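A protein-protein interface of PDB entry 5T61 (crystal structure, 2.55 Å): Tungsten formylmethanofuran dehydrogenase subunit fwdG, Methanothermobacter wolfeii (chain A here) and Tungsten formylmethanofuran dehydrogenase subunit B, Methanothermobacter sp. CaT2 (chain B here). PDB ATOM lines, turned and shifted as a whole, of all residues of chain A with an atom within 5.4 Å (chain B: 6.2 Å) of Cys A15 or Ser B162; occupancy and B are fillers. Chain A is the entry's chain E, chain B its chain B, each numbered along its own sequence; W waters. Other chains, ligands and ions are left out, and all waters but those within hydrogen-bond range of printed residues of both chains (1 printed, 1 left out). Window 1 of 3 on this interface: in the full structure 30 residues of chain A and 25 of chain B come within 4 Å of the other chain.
O of Cys A15 is in hydrogen-bond range of OG of Ser B162 (3.1 Å).
The guanidinium group (NE) of Arg B36 sits at hydrogen-bond distance from the backbone carbonyl oxygen (O) of Cys A12, 2.7 Å away.
The side-chain amide nitrogen (ND2) of Asn A17 is in hydrogen-bond range of the side-chain sulfur (SD) of Met B154, at 3.5 Å.
The backbone NH (N) of Arg B36 is in hydrogen-bond range of the backbone carbonyl oxygen (O) of His A13 (2.9 Å).
N of Ser B162 sits close to OD1 of Asn A17 (3.1 Å).
The backbone carbonyl oxygen of Cys A15 sits close to the backbone carbonyl oxygen of Pro B158.
ND1 of His A13 lies within hydrogen-bond range of O of Met B154 (2.9 Å).
Printed residues of chain B within 4 Å of Cys A15: Met B154, Pro B158, Arg B159 and Ser B162.
Of chain A, only Cys A15 (3.1 Å), Gly A16 (3.7 Å), Asn A17 (3.1 Å), Ile A20 (3.8 Å) and Gly A35 (3.6 Å) come within 4 Å of Ser B162.
Of the printed residues of chain B, Gly A16 touches Ser B162.
Printed residues of chain B within 4 Å of Ile A20: Ser B162 (3.8 Å) and Phe B166 (3.6 Å).
Of the printed residues of chain B, Asn A17 touches Met B154 (3.5 Å), Met B161 (3.9 Å), Ser B162 (3.1 Å) and Phe B166 (3.5 Å).
Printed residues of chain A within 4 Å of Phe B166: Asn A17 and Ile A20.
The nearest printed residue of chain A that does not touch Ser B162 is Cys A18 (6.1 Å).
Water W1 lies within hydrogen-bond range of the backbone carbonyl oxygen (O) of Gly A14 (2.7 Å) and the guanidinium group (NE) of Arg B159 (3.1 Å).
Hydrophobic or aromatic side chains of chain B within 4 Å of the printed part of chain A: Met B154, Met B161, Phe B166 and Ala B167.
Of the 10 printed residues of chain A, 8 touch a printed residue of chain B.
Among the printed residues, 20 pairs touch across the chains.
Cys B35 touches His A13 (CB to O, 3.6 Å).
Cys B35 touches Gly A14.
O of Gly A14 touches CG of Arg B159 (3.9 Å).
Cys A15 touches Arg B159 (O to CA, 3.4 Å).
Ser B162 touches Gly A16 (CB to C, 3.7 Å).
OD1 of Asn A17 touches C of Met B161, at 3.9 Å.
Asn A17 touches Phe B166.
Ile A20 touches Ser B162 (CG2 to O, 3.8 Å).
Ile A20 touches Phe B166.
Gly A35 touches Ala B167 (CA to CB, 3.6 Å).
ND2 of Asn A17 lies close to SG of Cys A15 (3.2 Å).
The backbone NH of Ala B167 sits at hydrogen-bond distance from the backbone carbonyl oxygen of Ser B162 (3.4 Å).
O of Met B161 lies within hydrogen-bond range of N of Phe B166, at 3.1 Å.
The side-chain hydroxyl (OG) of Ser B162 is in hydrogen-bond range of the backbone carbonyl oxygen (O) of Arg B159 (3.0 Å).
The backbone NH of Gly A14 sits close to the side-chain sulfur of Cys A12 (2.9 Å).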
ATOM      1  N   CYS A  12      22.112   1.220 -15.078  1.00  0.00           N
ATOM      2  CA  CYS A  12      22.583   1.557 -16.412  1.00  0.00           C
ATOM      3  C   CYS A  12      23.095   0.343 -17.183  1.00  0.00           C
ATOM      4  O   CYS A  12      23.688  -0.577 -16.616  1.00  0.00           O
ATOM      5  CB  CYS A  12      23.701   2.589 -16.308  1.00  0.00           C
ATOM      6  SG  CYS A  12      24.677   2.698 -17.794  1.00  0.00           S
ATOM      7  N   HIS A  13      22.878   0.368 -18.505  1.00  0.00           N
ATOM      8  CA  HIS A  13      23.368  -0.666 -19.412  1.00  0.00           C
ATOM      9  C   HIS A  13      24.659  -0.289 -20.127  1.00  0.00           C
ATOM     10  O   HIS A  13      25.275  -1.161 -20.753  1.00  0.00           O
ATOM     11  CB  HIS A  13      22.321  -0.986 -20.488  1.00  0.00           C
ATOM     12  CG  HIS A  13      21.107  -1.688 -19.973  1.00  0.00           C
ATOM     13  ND1 HIS A  13      20.359  -2.543 -20.753  1.00  0.00           N
ATOM     14  CD2 HIS A  13      20.498  -1.650 -18.764  1.00  0.00           C
ATOM     15  CE1 HIS A  13      19.348  -3.010 -20.043  1.00  0.00           C
ATOM     16  NE2 HIS A  13      19.409  -2.483 -18.834  1.00  0.00           N
ATOM     17  N   GLY A  14      25.070   0.976 -20.071  1.00  0.00           N
ATOM     18  CA  GLY A  14      26.172   1.418 -20.899  1.00  0.00           C
ATOM     19  C   GLY A  14      25.833   1.541 -22.367  1.00  0.00           C
ATOM     20  O   GLY A  14      26.741   1.556 -23.203  1.00  0.00           O
ATOM     21  N   CYS A  15      24.541   1.613 -22.715  1.00  0.00           N
ATOM     22  CA  CYS A  15      24.156   1.478 -24.117  1.00  0.00           C
ATOM     23  C   CYS A  15      24.551   2.707 -24.928  1.00  0.00           C
ATOM     24  O   CYS A  15      24.733   2.608 -26.146  1.00  0.00           O
ATOM     25  CB  CYS A  15      22.655   1.243 -24.254  1.00  0.00           C
ATOM     26  SG  CYS A  15      21.694   2.736 -24.461  1.00  0.00           S
ATOM     27  N   GLY A  16      24.640   3.872 -24.290  1.00  0.00           N
ATOM     28  CA  GLY A  16      25.115   5.067 -24.952  1.00  0.00           C
ATOM     29  C   GLY A  16      24.073   5.932 -25.633  1.00  0.00           C
ATOM     30  O   GLY A  16      24.452   6.931 -26.262  1.00  0.00           O
ATOM     31  N   ASN A  17      22.781   5.593 -25.543  1.00  0.00           N
ATOM     32  CA  ASN A  17      21.777   6.388 -26.248  1.00  0.00           C
ATOM     33  C   ASN A  17      21.758   7.825 -25.746  1.00  0.00           C
ATOM     34  O   ASN A  17      21.647   8.764 -26.542  1.00  0.00           O
ATOM     35  CB  ASN A  17      20.382   5.772 -26.113  1.00  0.00           C
ATOM     36  CG  ASN A  17      20.286   4.382 -26.708  1.00  0.00           C
ATOM     37  OD1 ASN A  17      21.116   3.980 -27.521  1.00  0.00           O
ATOM     38  ND2 ASN A  17      19.265   3.637 -26.302  1.00  0.00           N
ATOM     39  N   CYS A  18      21.861   8.019 -24.428  1.00  0.00           N
ATOM     40  CA  CYS A  18      21.849   9.374 -23.887  1.00  0.00           C
ATOM     41  C   CYS A  18      23.054  10.162 -24.377  1.00  0.00           C
ATOM     42  O   CYS A  18      22.933  11.342 -24.727  1.00  0.00           O
ATOM     43  CB  CYS A  18      21.855   9.350 -22.363  1.00  0.00           C
ATOM     44  SG  CYS A  18      23.485   8.965 -21.707  1.00  0.00           S
ATOM     45  N   ILE A  20      24.726   9.878 -27.124  1.00  0.00           N
ATOM     46  CA  ILE A  20      24.580  10.256 -28.524  1.00  0.00           C
ATOM     47  C   ILE A  20      23.437  11.248 -28.711  1.00  0.00           C
ATOM     48  O   ILE A  20      23.543  12.179 -29.513  1.00  0.00           O
ATOM     49  CB  ILE A  20      24.388   8.996 -29.387  1.00  0.00           C
ATOM     50  CG1 ILE A  20      25.517   7.994 -29.131  1.00  0.00           C
ATOM     51  CG2 ILE A  20      24.311   9.363 -30.859  1.00  0.00           C
ATOM     52  CD1 ILE A  20      26.904   8.570 -29.307  1.00  0.00           C
ATOM     53  N   GLY A  35      27.166   8.943 -33.543  1.00  0.00           N
ATOM     54  CA  GLY A  35      26.838   7.721 -32.838  1.00  0.00           C
ATOM     55  C   GLY A  35      27.993   6.946 -32.243  1.00  0.00           C
ATOM     56  O   GLY A  35      27.762   5.871 -31.670  1.00  0.00           O
ATOM     57  N   VAL A  48      29.970   7.041 -21.284  1.00  0.00           N
ATOM     58  CA  VAL A  48      29.962   5.703 -20.711  1.00  0.00           C
ATOM     59  C   VAL A  48      31.391   5.368 -20.312  1.00  0.00           C
ATOM     60  O   VAL A  48      32.308   5.407 -21.141  1.00  0.00           O
ATOM     61  CB  VAL A  48      29.409   4.676 -21.708  1.00  0.00           C
ATOM     62  CG1 VAL A  48      29.528   3.280 -21.138  1.00  0.00           C
ATOM     63  CG2 VAL A  48      27.960   4.991 -22.048  1.00  0.00           C
ATOM     64  N   CYS B  35      30.025  -0.920 -23.430  1.00  0.00           N
ATOM     65  CA  CYS B  35      28.811  -1.040 -22.640  1.00  0.00           C
ATOM     66  C   CYS B  35      29.076  -1.922 -21.425  1.00  0.00           C
ATOM     67  O   CYS B  35      30.196  -2.389 -21.197  1.00  0.00           O
ATOM     68  CB  CYS B  35      27.672  -1.631 -23.462  1.00  0.00           C
ATOM     69  SG  CYS B  35      27.633  -3.426 -23.352  1.00  0.00           S
ATOM     70  N   ARG B  36      28.018  -2.185 -20.651  1.00  0.00           N
ATOM     71  CA  ARG B  36      28.176  -2.946 -19.416  1.00  0.00           C
ATOM     72  C   ARG B  36      28.740  -4.337 -19.681  1.00  0.00           C
ATOM     73  O   ARG B  36      29.560  -4.839 -18.902  1.00  0.00           O
ATOM     74  CB  ARG B  36      26.843  -3.051 -18.675  1.00  0.00           C
ATOM     75  CG  ARG B  36      26.937  -3.901 -17.411  1.00  0.00           C
ATOM     76  CD  ARG B  36      25.636  -3.981 -16.625  1.00  0.00           C
ATOM     77  NE  ARG B  36      25.226  -2.707 -16.046  1.00  0.00           N
ATOM     78  CZ  ARG B  36      25.627  -2.271 -14.858  1.00  0.00           C
ATOM     79  NH1 ARG B  36      26.461  -3.003 -14.131  1.00  0.00           N
ATOM     80  NH2 ARG B  36      25.199  -1.105 -14.395  1.00  0.00           N
ATOM     81  N   MET B 154      18.911  -3.665 -26.540  1.00  0.00           N
ATOM     82  CA  MET B 154      19.270  -2.967 -25.308  1.00  0.00           C
ATOM     83  C   MET B 154      19.875  -3.932 -24.290  1.00  0.00           C
ATOM     84  O   MET B 154      20.704  -3.525 -23.468  1.00  0.00           O
ATOM     85  CB  MET B 154      18.044  -2.228 -24.715  1.00  0.00           C
ATOM     86  CG  MET B 154      17.550  -1.151 -25.672  1.00  0.00           C
ATOM     87  SD  MET B 154      18.671   0.240 -25.893  1.00  0.00           S
ATOM     88  CE  MET B 154      19.066   0.659 -24.217  1.00  0.00           C
ATOM     89  N   PRO B 158      23.976  -3.796 -26.692  1.00  0.00           N
ATOM     90  CA  PRO B 158      23.551  -2.561 -26.007  1.00  0.00           C
ATOM     91  C   PRO B 158      23.842  -1.277 -26.759  1.00  0.00           C
ATOM     92  O   PRO B 158      23.036  -0.342 -26.691  1.00  0.00           O
ATOM     93  CB  PRO B 158      24.325  -2.631 -24.686  1.00  0.00           C
ATOM     94  CG  PRO B 158      24.477  -4.097 -24.446  1.00  0.00           C
ATOM     95  CD  PRO B 158      24.739  -4.684 -25.801  1.00  0.00           C
ATOM     96  N   ARG B 159      24.936  -1.204 -27.506  1.00  0.00           N
ATOM     97  CA  ARG B 159      25.261   0.014 -28.230  1.00  0.00           C
ATOM     98  C   ARG B 159      24.728   0.011 -29.658  1.00  0.00           C
ATOM     99  O   ARG B 159      24.999   0.954 -30.403  1.00  0.00           O
ATOM    100  CB  ARG B 159      26.777   0.238 -28.240  1.00  0.00           C
ATOM    101  CG  ARG B 159      27.414   0.290 -26.860  1.00  0.00           C
ATOM    102  CD  ARG B 159      28.907   0.553 -26.965  1.00  0.00           C
ATOM    103  NE  ARG B 159      29.189   1.913 -27.416  1.00  0.00           N
ATOM    104  CZ  ARG B 159      30.294   2.272 -28.062  1.00  0.00           C
ATOM    105  NH1 ARG B 159      31.220   1.367 -28.340  1.00  0.00           N
ATOM    106  NH2 ARG B 159      30.472   3.532 -28.435  1.00  0.00           N
ATOM    107  N   HIS B 160      23.960  -1.012 -30.047  1.00  0.00           N
ATOM    108  CA  HIS B 160      23.498  -1.115 -31.430  1.00  0.00           C
ATOM    109  C   HIS B 160      22.592   0.050 -31.808  1.00  0.00           C
ATOM    110  O   HIS B 160      22.719   0.617 -32.898  1.00  0.00           O
ATOM    111  CB  HIS B 160      22.764  -2.443 -31.632  1.00  0.00           C
ATOM    112  CG  HIS B 160      22.669  -2.882 -33.062  1.00  0.00           C
ATOM    113  ND1 HIS B 160      21.664  -2.464 -33.907  1.00  0.00           N
ATOM    114  CD2 HIS B 160      23.445  -3.723 -33.787  1.00  0.00           C
ATOM    115  CE1 HIS B 160      21.828  -3.024 -35.093  1.00  0.00           C
ATOM    116  NE2 HIS B 160      22.901  -3.792 -35.047  1.00  0.00           N
ATOM    117  N   MET B 161      21.662   0.412 -30.921  1.00  0.00           N
ATOM    118  CA  MET B 161      20.726   1.491 -31.214  1.00  0.00           C
ATOM    119  C   MET B 161      21.423   2.844 -31.250  1.00  0.00           C
ATOM    120  O   MET B 161      21.170   3.656 -32.147  1.00  0.00           O
ATOM    121  CB  MET B 161      19.609   1.492 -30.174  1.00  0.00           C
ATOM    122  CG  MET B 161      18.781   0.226 -30.195  1.00  0.00           C
ATOM    123  SD  MET B 161      17.342   0.337 -29.127  1.00  0.00           S
ATOM    124  CE  MET B 161      16.308   1.415 -30.104  1.00  0.00           C
ATOM    125  N   SER B 162      22.313   3.098 -30.290  1.00  0.00           N
ATOM    126  CA  SER B 162      23.002   4.381 -30.247  1.00  0.00           C
ATOM    127  C   SER B 162      23.857   4.603 -31.485  1.00  0.00           C
ATOM    128  O   SER B 162      24.009   5.744 -31.940  1.00  0.00           O
ATOM    129  CB  SER B 162      23.854   4.469 -28.980  1.00  0.00           C
ATOM    130  OG  SER B 162      25.023   3.675 -29.091  1.00  0.00           O
ATOM    131  N   ARG B 163      24.433   3.538 -32.041  1.00  0.00           N
ATOM    132  CA  ARG B 163      25.290   3.709 -33.207  1.00  0.00           C
ATOM    133  C   ARG B 163      24.504   3.751 -34.518  1.00  0.00           C
ATOM    134  O   ARG B 163      24.953   4.385 -35.478  1.00  0.00           O
ATOM    135  CB  ARG B 163      26.359   2.615 -33.237  1.00  0.00           C
ATOM    136  CG  ARG B 163      27.100   2.484 -31.913  1.00  0.00           C
ATOM    137  CD  ARG B 163      28.532   2.023 -32.084  1.00  0.00           C
ATOM    138  NE  ARG B 163      28.677   0.828 -32.905  1.00  0.00           N
ATOM    139  CZ  ARG B 163      29.748   0.593 -33.654  1.00  0.00           C
ATOM    140  NH1 ARG B 163      30.641   1.559 -33.823  1.00  0.00           N
ATOM    141  NH2 ARG B 163      29.855  -0.529 -34.353  1.00  0.00           N
ATOM    142  N   ASN B 164      23.344   3.090 -34.595  1.00  0.00           N
ATOM    143  CA  ASN B 164      22.608   3.008 -35.853  1.00  0.00           C
ATOM    144  C   ASN B 164      21.300   3.791 -35.887  1.00  0.00           C
ATOM    145  O   ASN B 164      20.819   4.096 -36.983  1.00  0.00           O
ATOM    146  CB  ASN B 164      22.317   1.539 -36.218  1.00  0.00           C
ATOM    147  CG  ASN B 164      23.580   0.753 -36.542  1.00  0.00           C
ATOM    148  OD1 ASN B 164      24.405   1.187 -37.352  1.00  0.00           O
ATOM    149  ND2 ASN B 164      23.733  -0.410 -35.918  1.00  0.00           N
ATOM    150  N   VAL B 165      20.713   4.129 -34.741  1.00  0.00           N
ATOM    151  CA  VAL B 165      19.423   4.818 -34.695  1.00  0.00           C
ATOM    152  C   VAL B 165      19.577   6.256 -34.205  1.00  0.00           C
ATOM    153  O   VAL B 165      19.199   7.201 -34.898  1.00  0.00           O
ATOM    154  CB  VAL B 165      18.403   4.039 -33.836  1.00  0.00           C
ATOM    155  CG1 VAL B 165      17.080   4.790 -33.778  1.00  0.00           C
ATOM    156  CG2 VAL B 165      18.200   2.641 -34.402  1.00  0.00           C
ATOM    157  N   PHE B 166      20.136   6.441 -33.010  1.00  0.00           N
ATOM    158  CA  PHE B 166      20.325   7.786 -32.482  1.00  0.00           C
ATOM    159  C   PHE B 166      21.429   8.557 -33.197  1.00  0.00           C
ATOM    160  O   PHE B 166      21.524   9.775 -33.019  1.00  0.00           O
ATOM    161  CB  PHE B 166      20.609   7.718 -30.979  1.00  0.00           C
ATOM    162  CG  PHE B 166      19.401   7.364 -30.153  1.00  0.00           C
ATOM    163  CD1 PHE B 166      18.530   8.353 -29.711  1.00  0.00           C
ATOM    164  CD2 PHE B 166      19.131   6.046 -29.824  1.00  0.00           C
ATOM    165  CE1 PHE B 166      17.419   8.031 -28.960  1.00  0.00           C
ATOM    166  CE2 PHE B 166      18.017   5.717 -29.069  1.00  0.00           C
ATOM    167  CZ  PHE B 166      17.162   6.710 -28.637  1.00  0.00           C
ATOM    168  N   ALA B 167      22.260   7.882 -33.987  1.00  0.00           N
ATOM    169  CA  ALA B 167      23.352   8.547 -34.687  1.00  0.00           C
ATOM    170  C   ALA B 167      22.831   9.503 -35.752  1.00  0.00           C
ATOM    171  O   ALA B 167      21.823   9.238 -36.414  1.00  0.00           O
ATOM    172  CB  ALA B 167      24.270   7.512 -35.332  1.00  0.00           C
HETATM  173  O   HOH W   1      28.433   3.141 -24.636  1.00  0.00           O
